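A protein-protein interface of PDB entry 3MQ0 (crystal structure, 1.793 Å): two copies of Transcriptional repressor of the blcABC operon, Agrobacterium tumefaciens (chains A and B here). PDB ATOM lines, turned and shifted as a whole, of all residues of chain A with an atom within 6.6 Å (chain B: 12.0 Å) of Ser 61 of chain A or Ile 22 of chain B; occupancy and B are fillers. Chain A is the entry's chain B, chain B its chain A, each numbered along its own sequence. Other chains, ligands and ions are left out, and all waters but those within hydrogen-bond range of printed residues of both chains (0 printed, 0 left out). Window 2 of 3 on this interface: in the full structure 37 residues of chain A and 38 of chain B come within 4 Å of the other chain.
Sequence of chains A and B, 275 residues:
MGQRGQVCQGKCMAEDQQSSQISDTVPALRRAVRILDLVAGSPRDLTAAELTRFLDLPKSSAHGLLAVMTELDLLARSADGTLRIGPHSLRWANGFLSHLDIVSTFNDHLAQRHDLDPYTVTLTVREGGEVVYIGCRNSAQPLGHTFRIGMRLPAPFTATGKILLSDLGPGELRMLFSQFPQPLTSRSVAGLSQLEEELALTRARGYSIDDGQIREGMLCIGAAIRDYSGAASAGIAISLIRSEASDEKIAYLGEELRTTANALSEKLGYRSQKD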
ATOM      1  N   VAL A  26     -23.040 -18.302  24.913  1.00  0.00           N
ATOM      2  CA  VAL A  26     -23.010 -16.832  24.968  1.00  0.00           C
ATOM      3  C   VAL A  26     -23.396 -16.167  23.643  1.00  0.00           C
ATOM      4  O   VAL A  26     -22.602 -15.450  23.046  1.00  0.00           O
ATOM      5  CB  VAL A  26     -21.646 -16.305  25.443  1.00  0.00           C
ATOM      6  CG1 VAL A  26     -21.792 -14.874  25.942  1.00  0.00           C
ATOM      7  CG2 VAL A  26     -21.120 -17.184  26.573  1.00  0.00           C
ATOM      8  N   PRO A  27     -24.620 -16.426  23.168  1.00  0.00           N
ATOM      9  CA  PRO A  27     -25.100 -15.978  21.857  1.00  0.00           C
ATOM     10  C   PRO A  27     -24.900 -14.500  21.551  1.00  0.00           C
ATOM     11  O   PRO A  27     -24.484 -14.185  20.438  1.00  0.00           O
ATOM     12  CB  PRO A  27     -26.598 -16.284  21.919  1.00  0.00           C
ATOM     13  CG  PRO A  27     -26.718 -17.387  22.859  1.00  0.00           C
ATOM     14  CD  PRO A  27     -25.614 -17.263  23.861  1.00  0.00           C
ATOM     15  N   ALA A  28     -25.195 -13.603  22.496  1.00  0.00           N
ATOM     16  CA  ALA A  28     -25.091 -12.163  22.221  1.00  0.00           C
ATOM     17  C   ALA A  28     -23.652 -11.745  21.897  1.00  0.00           C
ATOM     18  O   ALA A  28     -23.407 -10.913  21.024  1.00  0.00           O
ATOM     19  CB  ALA A  28     -25.643 -11.347  23.405  1.00  0.00           C
ATOM     20  N   LEU A  29     -22.696 -12.348  22.584  1.00  0.00           N
ATOM     21  CA  LEU A  29     -21.299 -12.079  22.298  1.00  0.00           C
ATOM     22  C   LEU A  29     -20.902 -12.580  20.902  1.00  0.00           C
ATOM     23  O   LEU A  29     -20.227 -11.872  20.160  1.00  0.00           O
ATOM     24  CB  LEU A  29     -20.403 -12.709  23.364  1.00  0.00           C
ATOM     25  CG  LEU A  29     -18.919 -12.444  23.175  1.00  0.00           C
ATOM     26  CD1 LEU A  29     -18.635 -10.950  23.051  1.00  0.00           C
ATOM     27  CD2 LEU A  29     -18.195 -13.051  24.375  1.00  0.00           C
ATOM     28  N   ARG A  31     -22.798 -12.977  18.271  1.00  0.00           N
ATOM     29  CA  ARG A  31     -23.386 -12.099  17.263  1.00  0.00           C
ATOM     30  C   ARG A  31     -22.686 -10.740  17.209  1.00  0.00           C
ATOM     31  O   ARG A  31     -22.490 -10.192  16.125  1.00  0.00           O
ATOM     32  CB  ARG A  31     -24.894 -11.885  17.482  1.00  0.00           C
ATOM     33  CG  ARG A  31     -25.757 -13.158  17.519  1.00  0.00           C
ATOM     34  CD  ARG A  31     -25.345 -14.169  16.494  1.00  0.00           C
ATOM     35  NE  ARG A  31     -26.258 -15.312  16.466  1.00  0.00           N
ATOM     36  CZ  ARG A  31     -26.209 -16.347  17.303  1.00  0.00           C
ATOM     37  NH1 ARG A  31     -25.300 -16.393  18.266  1.00  0.00           N
ATOM     38  NH2 ARG A  31     -27.079 -17.344  17.179  1.00  0.00           N
ATOM     39  N   LEU A  55     -27.637 -11.212  10.177  1.00  0.00           N
ATOM     40  CA  LEU A  55     -27.887 -11.781  11.496  1.00  0.00           C
ATOM     41  C   LEU A  55     -29.044 -12.774  11.474  1.00  0.00           C
ATOM     42  O   LEU A  55     -30.072 -12.539  10.836  1.00  0.00           O
ATOM     43  CB  LEU A  55     -28.175 -10.676  12.517  1.00  0.00           C
ATOM     44  CG  LEU A  55     -27.012  -9.771  12.937  1.00  0.00           C
ATOM     45  CD1 LEU A  55     -27.520  -8.530  13.671  1.00  0.00           C
ATOM     46  CD2 LEU A  55     -26.042 -10.533  13.810  1.00  0.00           C
ATOM     47  N   ASP A  56     -28.875 -13.884  12.178  1.00  0.00           N
ATOM     48  CA  ASP A  56     -29.938 -14.869  12.316  1.00  0.00           C
ATOM     49  C   ASP A  56     -30.918 -14.515  13.439  1.00  0.00           C
ATOM     50  O   ASP A  56     -31.228 -15.363  14.289  1.00  0.00           O
ATOM     51  CB  ASP A  56     -29.334 -16.251  12.568  1.00  0.00           C
ATOM     52  CG  ASP A  56     -28.517 -16.308  13.853  1.00  0.00           C
ATOM     53  OD1 ASP A  56     -28.046 -15.245  14.327  1.00  0.00           O
ATOM     54  OD2 ASP A  56     -28.355 -17.426  14.390  1.00  0.00           O
ATOM     55  N   LEU A  57     -31.400 -13.273  13.443  1.00  0.00           N
ATOM     56  CA  LEU A  57     -32.312 -12.787  14.480  1.00  0.00           C
ATOM     57  C   LEU A  57     -33.514 -12.075  13.877  1.00  0.00           C
ATOM     58  O   LEU A  57     -33.399 -11.455  12.820  1.00  0.00           O
ATOM     59  CB  LEU A  57     -31.590 -11.782  15.383  1.00  0.00           C
ATOM     60  CG  LEU A  57     -30.257 -12.185  16.011  1.00  0.00           C
ATOM     61  CD1 LEU A  57     -29.606 -10.964  16.631  1.00  0.00           C
ATOM     62  CD2 LEU A  57     -30.462 -13.268  17.032  1.00  0.00           C
ATOM     63  N   PRO A  58     -34.664 -12.125  14.567  1.00  0.00           N
ATOM     64  CA  PRO A  58     -35.792 -11.305  14.129  1.00  0.00           C
ATOM     65  C   PRO A  58     -35.296  -9.875  13.993  1.00  0.00           C
ATOM     66  O   PRO A  58     -34.355  -9.500  14.685  1.00  0.00           O
ATOM     67  CB  PRO A  58     -36.769 -11.391  15.304  1.00  0.00           C
ATOM     68  CG  PRO A  58     -36.378 -12.608  16.057  1.00  0.00           C
ATOM     69  CD  PRO A  58     -34.913 -12.782  15.863  1.00  0.00           C
ATOM     70  N   LYS A  59     -35.921  -9.096  13.121  1.00  0.00           N
ATOM     71  CA  LYS A  59     -35.508  -7.716  12.881  1.00  0.00           C
ATOM     72  C   LYS A  59     -35.421  -6.871  14.143  1.00  0.00           C
ATOM     73  O   LYS A  59     -34.468  -6.132  14.318  1.00  0.00           O
ATOM     74  CB  LYS A  59     -36.432  -7.043  11.862  1.00  0.00           C
ATOM     75  CG  LYS A  59     -36.232  -7.548  10.453  1.00  0.00           C
ATOM     76  CD  LYS A  59     -37.090  -6.791   9.458  1.00  0.00           C
ATOM     77  CE  LYS A  59     -36.997  -7.425   8.080  1.00  0.00           C
ATOM     78  NZ  LYS A  59     -35.573  -7.591   7.661  1.00  0.00           N
ATOM     79  N   SER A  60     -36.409  -6.980  15.022  1.00  0.00           N
ATOM     80  CA  SER A  60     -36.422  -6.138  16.218  1.00  0.00           C
ATOM     81  C   SER A  60     -35.259  -6.445  17.152  1.00  0.00           C
ATOM     82  O   SER A  60     -34.709  -5.550  17.801  1.00  0.00           O
ATOM     83  CB  SER A  60     -37.765  -6.244  16.957  1.00  0.00           C
ATOM     84  OG  SER A  60     -38.121  -7.596  17.193  1.00  0.00           O
ATOM     85  N   SER A  61     -34.885  -7.715  17.228  1.00  0.00           N
ATOM     86  CA  SER A  61     -33.784  -8.129  18.075  1.00  0.00           C
ATOM     87  C   SER A  61     -32.451  -7.701  17.472  1.00  0.00           C
ATOM     88  O   SER A  61     -31.535  -7.286  18.179  1.00  0.00           O
ATOM     89  CB  SER A  61     -33.833  -9.643  18.295  1.00  0.00           C
ATOM     90  OG  SER A  61     -32.682 -10.084  18.981  1.00  0.00           O
ATOM     91  N   ALA A  62     -32.345  -7.788  16.152  1.00  0.00           N
ATOM     92  CA  ALA A  62     -31.126  -7.367  15.494  1.00  0.00           C
ATOM     93  C   ALA A  62     -30.919  -5.870  15.722  1.00  0.00           C
ATOM     94  O   ALA A  62     -29.838  -5.450  16.113  1.00  0.00           O
ATOM     95  CB  ALA A  62     -31.163  -7.715  14.000  1.00  0.00           C
ATOM     96  N   HIS A  63     -31.952  -5.070  15.493  1.00  0.00           N
ATOM     97  CA  HIS A  63     -31.845  -3.632  15.723  1.00  0.00           C
ATOM     98  C   HIS A  63     -31.513  -3.299  17.175  1.00  0.00           C
ATOM     99  O   HIS A  63     -30.728  -2.398  17.446  1.00  0.00           O
ATOM    100  CB  HIS A  63     -33.122  -2.910  15.301  1.00  0.00           C
ATOM    101  CG  HIS A  63     -33.364  -2.939  13.819  1.00  0.00           C
ATOM    102  ND1 HIS A  63     -34.408  -2.269  13.222  1.00  0.00           N
ATOM    103  CD2 HIS A  63     -32.693  -3.559  12.820  1.00  0.00           C
ATOM    104  CE1 HIS A  63     -34.370  -2.474  11.916  1.00  0.00           C
ATOM    105  NE2 HIS A  63     -33.337  -3.252  11.646  1.00  0.00           N
ATOM    106  N   GLY A  64     -32.121  -4.017  18.105  1.00  0.00           N
ATOM    107  CA  GLY A  64     -31.844  -3.801  19.519  1.00  0.00           C
ATOM    108  C   GLY A  64     -30.402  -4.128  19.861  1.00  0.00           C
ATOM    109  O   GLY A  64     -29.768  -3.427  20.629  1.00  0.00           O
ATOM    110  N   LEU A  65     -29.869  -5.193  19.274  1.00  0.00           N
ATOM    111  CA  LEU A  65     -28.485  -5.560  19.550  1.00  0.00           C
ATOM    112  C   LEU A  65     -27.544  -4.488  19.024  1.00  0.00           C
ATOM    113  O   LEU A  65     -26.613  -4.083  19.720  1.00  0.00           O
ATOM    114  CB  LEU A  65     -28.146  -6.927  18.954  1.00  0.00           C
ATOM    115  CG  LEU A  65     -26.702  -7.404  19.080  1.00  0.00           C
ATOM    116  CD1 LEU A  65     -26.270  -7.527  20.544  1.00  0.00           C
ATOM    117  CD2 LEU A  65     -26.623  -8.743  18.369  1.00  0.00           C
ATOM    118  N   LEU A  66     -27.801  -4.020  17.803  1.00  0.00           N
ATOM    119  CA  LEU A  66     -26.972  -2.975  17.211  1.00  0.00           C
ATOM    120  C   LEU A  66     -27.015  -1.709  18.072  1.00  0.00           C
ATOM    121  O   LEU A  66     -26.004  -1.051  18.257  1.00  0.00           O
ATOM    122  CB  LEU A  66     -27.395  -2.677  15.770  1.00  0.00           C
ATOM    123  CG  LEU A  66     -27.176  -3.780  14.728  1.00  0.00           C
ATOM    124  CD1 LEU A  66     -27.754  -3.356  13.375  1.00  0.00           C
ATOM    125  CD2 LEU A  66     -25.706  -4.110  14.592  1.00  0.00           C
ATOM    126  N   SER B  20     -36.170 -11.810  23.581  1.00  0.00           N
ATOM    127  CA  SER B  20     -36.127 -12.569  24.823  1.00  0.00           C
ATOM    128  C   SER B  20     -35.142 -13.734  24.744  1.00  0.00           C
ATOM    129  O   SER B  20     -34.954 -14.457  25.726  1.00  0.00           O
ATOM    130  CB  SER B  20     -37.517 -13.071  25.186  1.00  0.00           C
ATOM    131  N   GLN B  21     -34.522 -13.927  23.583  1.00  0.00           N
ATOM    132  CA  GLN B  21     -33.504 -14.966  23.442  1.00  0.00           C
ATOM    133  C   GLN B  21     -32.111 -14.369  23.542  1.00  0.00           C
ATOM    134  O   GLN B  21     -31.380 -14.633  24.500  1.00  0.00           O
ATOM    135  CB  GLN B  21     -33.658 -15.732  22.126  1.00  0.00           C
ATOM    136  CG  GLN B  21     -34.566 -16.955  22.216  1.00  0.00           C
ATOM    137  CD  GLN B  21     -33.930 -18.113  22.969  1.00  0.00           C
ATOM    138  OE1 GLN B  21     -34.591 -19.111  23.264  1.00  0.00           O
ATOM    139  NE2 GLN B  21     -32.639 -17.989  23.274  1.00  0.00           N
ATOM    140  N   ILE B  22     -31.755 -13.555  22.553  1.00  0.00           N
ATOM    141  CA  ILE B  22     -30.469 -12.873  22.546  1.00  0.00           C
ATOM    142  C   ILE B  22     -30.336 -11.933  23.754  1.00  0.00           C
ATOM    143  O   ILE B  22     -29.238 -11.715  24.275  1.00  0.00           O
ATOM    144  CB  ILE B  22     -30.283 -12.077  21.234  1.00  0.00           C
ATOM    145  CG1 ILE B  22     -28.813 -11.801  20.976  1.00  0.00           C
ATOM    146  CG2 ILE B  22     -31.080 -10.790  21.263  1.00  0.00           C
ATOM    147  CD1 ILE B  22     -28.094 -12.988  20.370  1.00  0.00           C
ATOM    148  N   SER B  23     -31.449 -11.383  24.221  1.00  0.00           N
ATOM    149  CA  SER B  23     -31.374 -10.434  25.335  1.00  0.00           C
ATOM    150  C   SER B  23     -30.873 -11.105  26.608  1.00  0.00           C
ATOM    151  O   SER B  23     -30.260 -10.463  27.448  1.00  0.00           O
ATOM    152  CB  SER B  23     -32.712  -9.725  25.574  1.00  0.00           C
ATOM    153  OG  SER B  23     -33.725 -10.639  25.948  1.00  0.00           O
ATOM    154  N   ASP B  24     -31.101 -12.412  26.730  1.00  0.00           N
ATOM    155  CA  ASP B  24     -30.619 -13.157  27.893  1.00  0.00           C
ATOM    156  C   ASP B  24     -29.102 -13.140  28.083  1.00  0.00           C
ATOM    157  O   ASP B  24     -28.612 -13.343  29.191  1.00  0.00           O
ATOM    158  CB  ASP B  24     -31.127 -14.603  27.846  1.00  0.00           C
ATOM    159  CG  ASP B  24     -32.631 -14.679  28.003  1.00  0.00           C
ATOM    160  OD1 ASP B  24     -33.194 -13.703  28.543  1.00  0.00           O
ATOM    161  OD2 ASP B  24     -33.243 -15.692  27.595  1.00  0.00           O
ATOM    162  N   THR B  25     -28.348 -12.902  27.017  1.00  0.00           N
ATOM    163  CA  THR B  25     -26.905 -12.819  27.176  1.00  0.00           C
ATOM    164  C   THR B  25     -26.325 -11.454  26.828  1.00  0.00           C
ATOM    165  O   THR B  25     -25.102 -11.286  26.748  1.00  0.00           O
ATOM    166  CB  THR B  25     -26.164 -13.948  26.423  1.00  0.00           C
ATOM    167  OG1 THR B  25     -26.643 -14.034  25.074  1.00  0.00           O
ATOM    168  CG2 THR B  25     -26.406 -15.280  27.127  1.00  0.00           C
ATOM    169  N   VAL B  26     -27.195 -10.465  26.652  1.00  0.00           N
ATOM    170  CA  VAL B  26     -26.726  -9.087  26.515  1.00  0.00           C
ATOM    171  C   VAL B  26     -25.837  -8.619  27.694  1.00  0.00           C
ATOM    172  O   VAL B  26     -24.829  -7.941  27.472  1.00  0.00           O
ATOM    173  CB  VAL B  26     -27.916  -8.111  26.227  1.00  0.00           C
ATOM    174  CG1 VAL B  26     -27.545  -6.665  26.535  1.00  0.00           C
ATOM    175  CG2 VAL B  26     -28.361  -8.268  24.764  1.00  0.00           C
ATOM    176  N   PRO B  27     -26.159  -9.023  28.936  1.00  0.00           N
ATOM    177  CA  PRO B  27     -25.260  -8.594  30.017  1.00  0.00           C
ATOM    178  C   PRO B  27     -23.823  -9.086  29.809  1.00  0.00           C
ATOM    179  O   PRO B  27     -22.889  -8.437  30.272  1.00  0.00           O
ATOM    180  CB  PRO B  27     -25.886  -9.223  31.266  1.00  0.00           C
ATOM    181  CG  PRO B  27     -27.349  -9.256  30.955  1.00  0.00           C
ATOM    182  CD  PRO B  27     -27.392  -9.635  29.465  1.00  0.00           C
ATOM    183  N   ALA B  28     -23.644 -10.190  29.091  1.00  0.00           N
ATOM    184  CA  ALA B  28     -22.291 -10.673  28.796  1.00  0.00           C
ATOM    185  C   ALA B  28     -21.495  -9.687  27.933  1.00  0.00           C
ATOM    186  O   ALA B  28     -20.262  -9.657  27.987  1.00  0.00           O
ATOM    187  CB  ALA B  28     -22.341 -12.038  28.138  1.00  0.00           C
ATOM    188  N   LEU B  29     -22.190  -8.858  27.165  1.00  0.00           N
ATOM    189  CA  LEU B  29     -21.521  -7.842  26.356  1.00  0.00           C
ATOM    190  C   LEU B  29     -20.769  -6.819  27.197  1.00  0.00           C
ATOM    191  O   LEU B  29     -19.597  -6.593  26.952  1.00  0.00           O
ATOM    192  CB  LEU B  29     -22.503  -7.115  25.433  1.00  0.00           C
ATOM    193  CG  LEU B  29     -23.006  -7.921  24.238  1.00  0.00           C
ATOM    194  CD1 LEU B  29     -23.892  -7.063  23.336  1.00  0.00           C
ATOM    195  CD2 LEU B  29     -21.819  -8.452  23.460  1.00  0.00           C
ATOM    196  N   ARG B  30     -21.445  -6.156  28.140  1.00  0.00           N
ATOM    197  CA  ARG B  30     -20.748  -5.220  29.008  1.00  0.00           C
ATOM    198  C   ARG B  30     -19.652  -5.952  29.773  1.00  0.00           C
ATOM    199  O   ARG B  30     -18.593  -5.399  30.000  1.00  0.00           O
ATOM    200  CB  ARG B  30     -21.691  -4.506  30.002  1.00  0.00           C
ATOM    201  CG  ARG B  30     -20.974  -3.732  31.151  1.00  0.00           C
ATOM    202  CD  ARG B  30     -20.204  -2.454  30.720  1.00  0.00           C
ATOM    203  NE  ARG B  30     -21.092  -1.410  30.222  1.00  0.00           N
ATOM    204  CZ  ARG B  30     -20.691  -0.362  29.502  1.00  0.00           C
ATOM    205  NH1 ARG B  30     -19.404  -0.212  29.201  1.00  0.00           N
ATOM    206  NH2 ARG B  30     -21.576   0.536  29.081  1.00  0.00           N
ATOM    207  N   ARG B  31     -19.928  -7.178  30.210  1.00  0.00           N
ATOM    208  CA  ARG B  31     -18.931  -7.903  31.007  1.00  0.00           C
ATOM    209  C   ARG B  31     -17.687  -8.147  30.169  1.00  0.00           C
ATOM    210  O   ARG B  31     -16.567  -7.974  30.646  1.00  0.00           O
ATOM    211  CB  ARG B  31     -19.506  -9.216  31.554  1.00  0.00           C
ATOM    212  CG  ARG B  31     -20.494  -9.010  32.689  1.00  0.00           C
ATOM    213  CD  ARG B  31     -21.190 -10.310  33.086  1.00  0.00           C
ATOM    214  NE  ARG B  31     -22.356 -10.024  33.922  1.00  0.00           N
ATOM    215  CZ  ARG B  31     -23.208 -10.948  34.346  1.00  0.00           C
ATOM    216  NH1 ARG B  31     -23.020 -12.221  34.016  1.00  0.00           N
ATOM    217  NH2 ARG B  31     -24.242 -10.597  35.096  1.00  0.00           N
ATOM    218  N   LEU B  65     -18.012 -17.378  29.932  1.00  0.00           N
ATOM    219  CA  LEU B  65     -17.744 -16.176  29.170  1.00  0.00           C
ATOM    220  C   LEU B  65     -16.286 -16.111  28.743  1.00  0.00           C
ATOM    221  O   LEU B  65     -15.994 -15.851  27.582  1.00  0.00           O
ATOM    222  CB  LEU B  65     -18.131 -14.928  29.972  1.00  0.00           C
ATOM    223  CG  LEU B  65     -17.812 -13.560  29.368  1.00  0.00           C
ATOM    224  CD1 LEU B  65     -18.491 -13.399  28.006  1.00  0.00           C
ATOM    225  CD2 LEU B  65     -18.271 -12.462  30.315  1.00  0.00           C
ATOM    226  N   VAL B  68     -15.573 -18.528  25.811  1.00  0.00           N
ATOM    227  CA  VAL B  68     -15.949 -18.009  24.490  1.00  0.00           C
ATOM    228  C   VAL B  68     -15.027 -16.875  24.030  1.00  0.00           C
ATOM    229  O   VAL B  68     -14.643 -16.823  22.864  1.00  0.00           O
ATOM    230  CB  VAL B  68     -17.432 -17.558  24.435  1.00  0.00           C
ATOM    231  CG1 VAL B  68     -17.742 -16.911  23.094  1.00  0.00           C
ATOM    232  CG2 VAL B  68     -18.345 -18.757  24.669  1.00  0.00           C
ATOM    233  N   LEU B  72     -12.897 -17.169  20.510  1.00  0.00           N
ATOM    234  CA  LEU B  72     -12.974 -16.165  19.456  1.00  0.00           C
ATOM    235  C   LEU B  72     -11.713 -15.307  19.361  1.00  0.00           C
ATOM    236  O   LEU B  72     -11.690 -14.316  18.635  1.00  0.00           O
ATOM    237  CB  LEU B  72     -14.173 -15.246  19.690  1.00  0.00           C
ATOM    238  CG  LEU B  72     -15.531 -15.941  19.744  1.00  0.00           C
ATOM    239  CD1 LEU B  72     -16.608 -14.899  19.986  1.00  0.00           C
ATOM    240  CD2 LEU B  72     -15.783 -16.728  18.455  1.00  0.00           C
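Ser 61 of chain A touches one residue of chain B. Of chain A, only Pro 27 (3.7 Å), Ala 28 (3.6 Å), Arg 31 (3.7 Å) and Ser 61 (2.9 Å) come within 4 Å of Ile 22 of chain B. Pro 27 of chain A touches just these residues of chain B: Ile 22 (3.7 Å) and Thr 25 (3.6 Å). Of the printed residues of chain B, Ala 28 of chain A touches Ile 22 (3.6 Å), Thr 25 (3.0 Å), Val 26 (3.7 Å) and Leu 29 (3.8 Å). Arg 31 of chain A touches just one residue of chain B: Ile 22 (3.7 Å). No residue of chain B comes within 4 Å of Pro 58 of chain A. No residue of chain B comes within 4 Å of Ser 60 of chain A. Ala 62 of chain A touches none of the printed residues of chain B. No residue of chain B comes within 4 Å of His 63 of chain A. Of the printed residues of chain B, Leu 65 of chain A touches Leu 29. Of the printed residues of chain A, Leu 65 of chain B touches Leu 29. Printed residues of chain A within 4 Å of Ala 28 of chain B: Val 26. Printed residues of chain A within 4 Å of Leu 29 of chain B: Ala 28, Leu 29 and Leu 65. Ser 20 of chain B touches none of the printed residues of chain A. The nearest residue of chain B that does not touch Ser 61 of chain A is Ser 23 of chain B (5.5 Å). The nearest residue of chain A that does not touch Ile 22 of chain B is Leu 57 of chain A (4.1 Å). The nearest printed residue of chain A that does not touch Val 68 of chain B is Leu 29 of chain A (4.1 Å).
O of Pro 27 of chain A is in hydrogen-bond range of NH1 of Arg 31 of chain A (3.2 Å). NE of Arg 31 of chain A lies within salt-bridge range of OD1 of Asp 56 of chain A, at 2.8 Å.
CB of Ala 28 of chain B touches CG1 of Val 26 of chain A, 3.6 Å away. Val 26 of chain A touches Val 68 of chain B. Ile 22 of chain B touches Pro 27 of chain A. CD of Pro 27 of chain A touches OG1 of Thr 25 of chain B, at 3.6 Å. Ile 22 of chain B touches Ala 28 of chain A (CD1 to CA, 3.6 Å). Ala 28 of chain A touches Val 26 of chain B (CB to N, 3.7 Å). Leu 29 of chain B touches Ala 28 of chain A. Leu 29 of chain B touches Leu 29 of chain A (CD2 to CA, 3.8 Å). Leu 29 of chain A touches Leu 65 of chain B (CD2 to CD1, 3.7 Å). CD1 of Leu 65 of chain A touches CD1 of Leu 29 of chain B (3.7 Å).
Of the 17 printed residues of chain A, 7 touch a printed residue of chain B. Printed residues of chain A that touch a printed residue of chain B: Val 26, Pro 27, Ala 28, Leu 29, Arg 31, Ser 61 and Leu 65. Hydrophobic or aromatic side chains of chain A that line the printed part of chain B: Val 26, Pro 27, Ala 28, Leu 29 and Leu 65. Of the 15 printed residues of chain B, 7 touch a printed residue of chain A.
Val 26 of chain A touches Ala 28 of chain B, and with the chains exchanged Ala 28 of chain A touches Val 26 of chain B. Ala 28 of chain A touches Leu 29 of chain B, but with the chains exchanged Leu 29 of chain A does not touch Ala 28 of chain B (5.2 Å). Leu 29 of chain B touches its own counterpart, Leu 29 of chain A. Leu 29 of chain A touches Leu 65 of chain B, and with the chains exchanged Leu 65 of chain A touches Leu 29 of chain B. Positions printed for both chains: 26, 27, 28, 29, 31 and 65.
The side-chain hydroxyl (OG1) of Thr 25 of chain B lies within hydrogen-bond range of the backbone NH (N) of Ala 28 of chain A.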
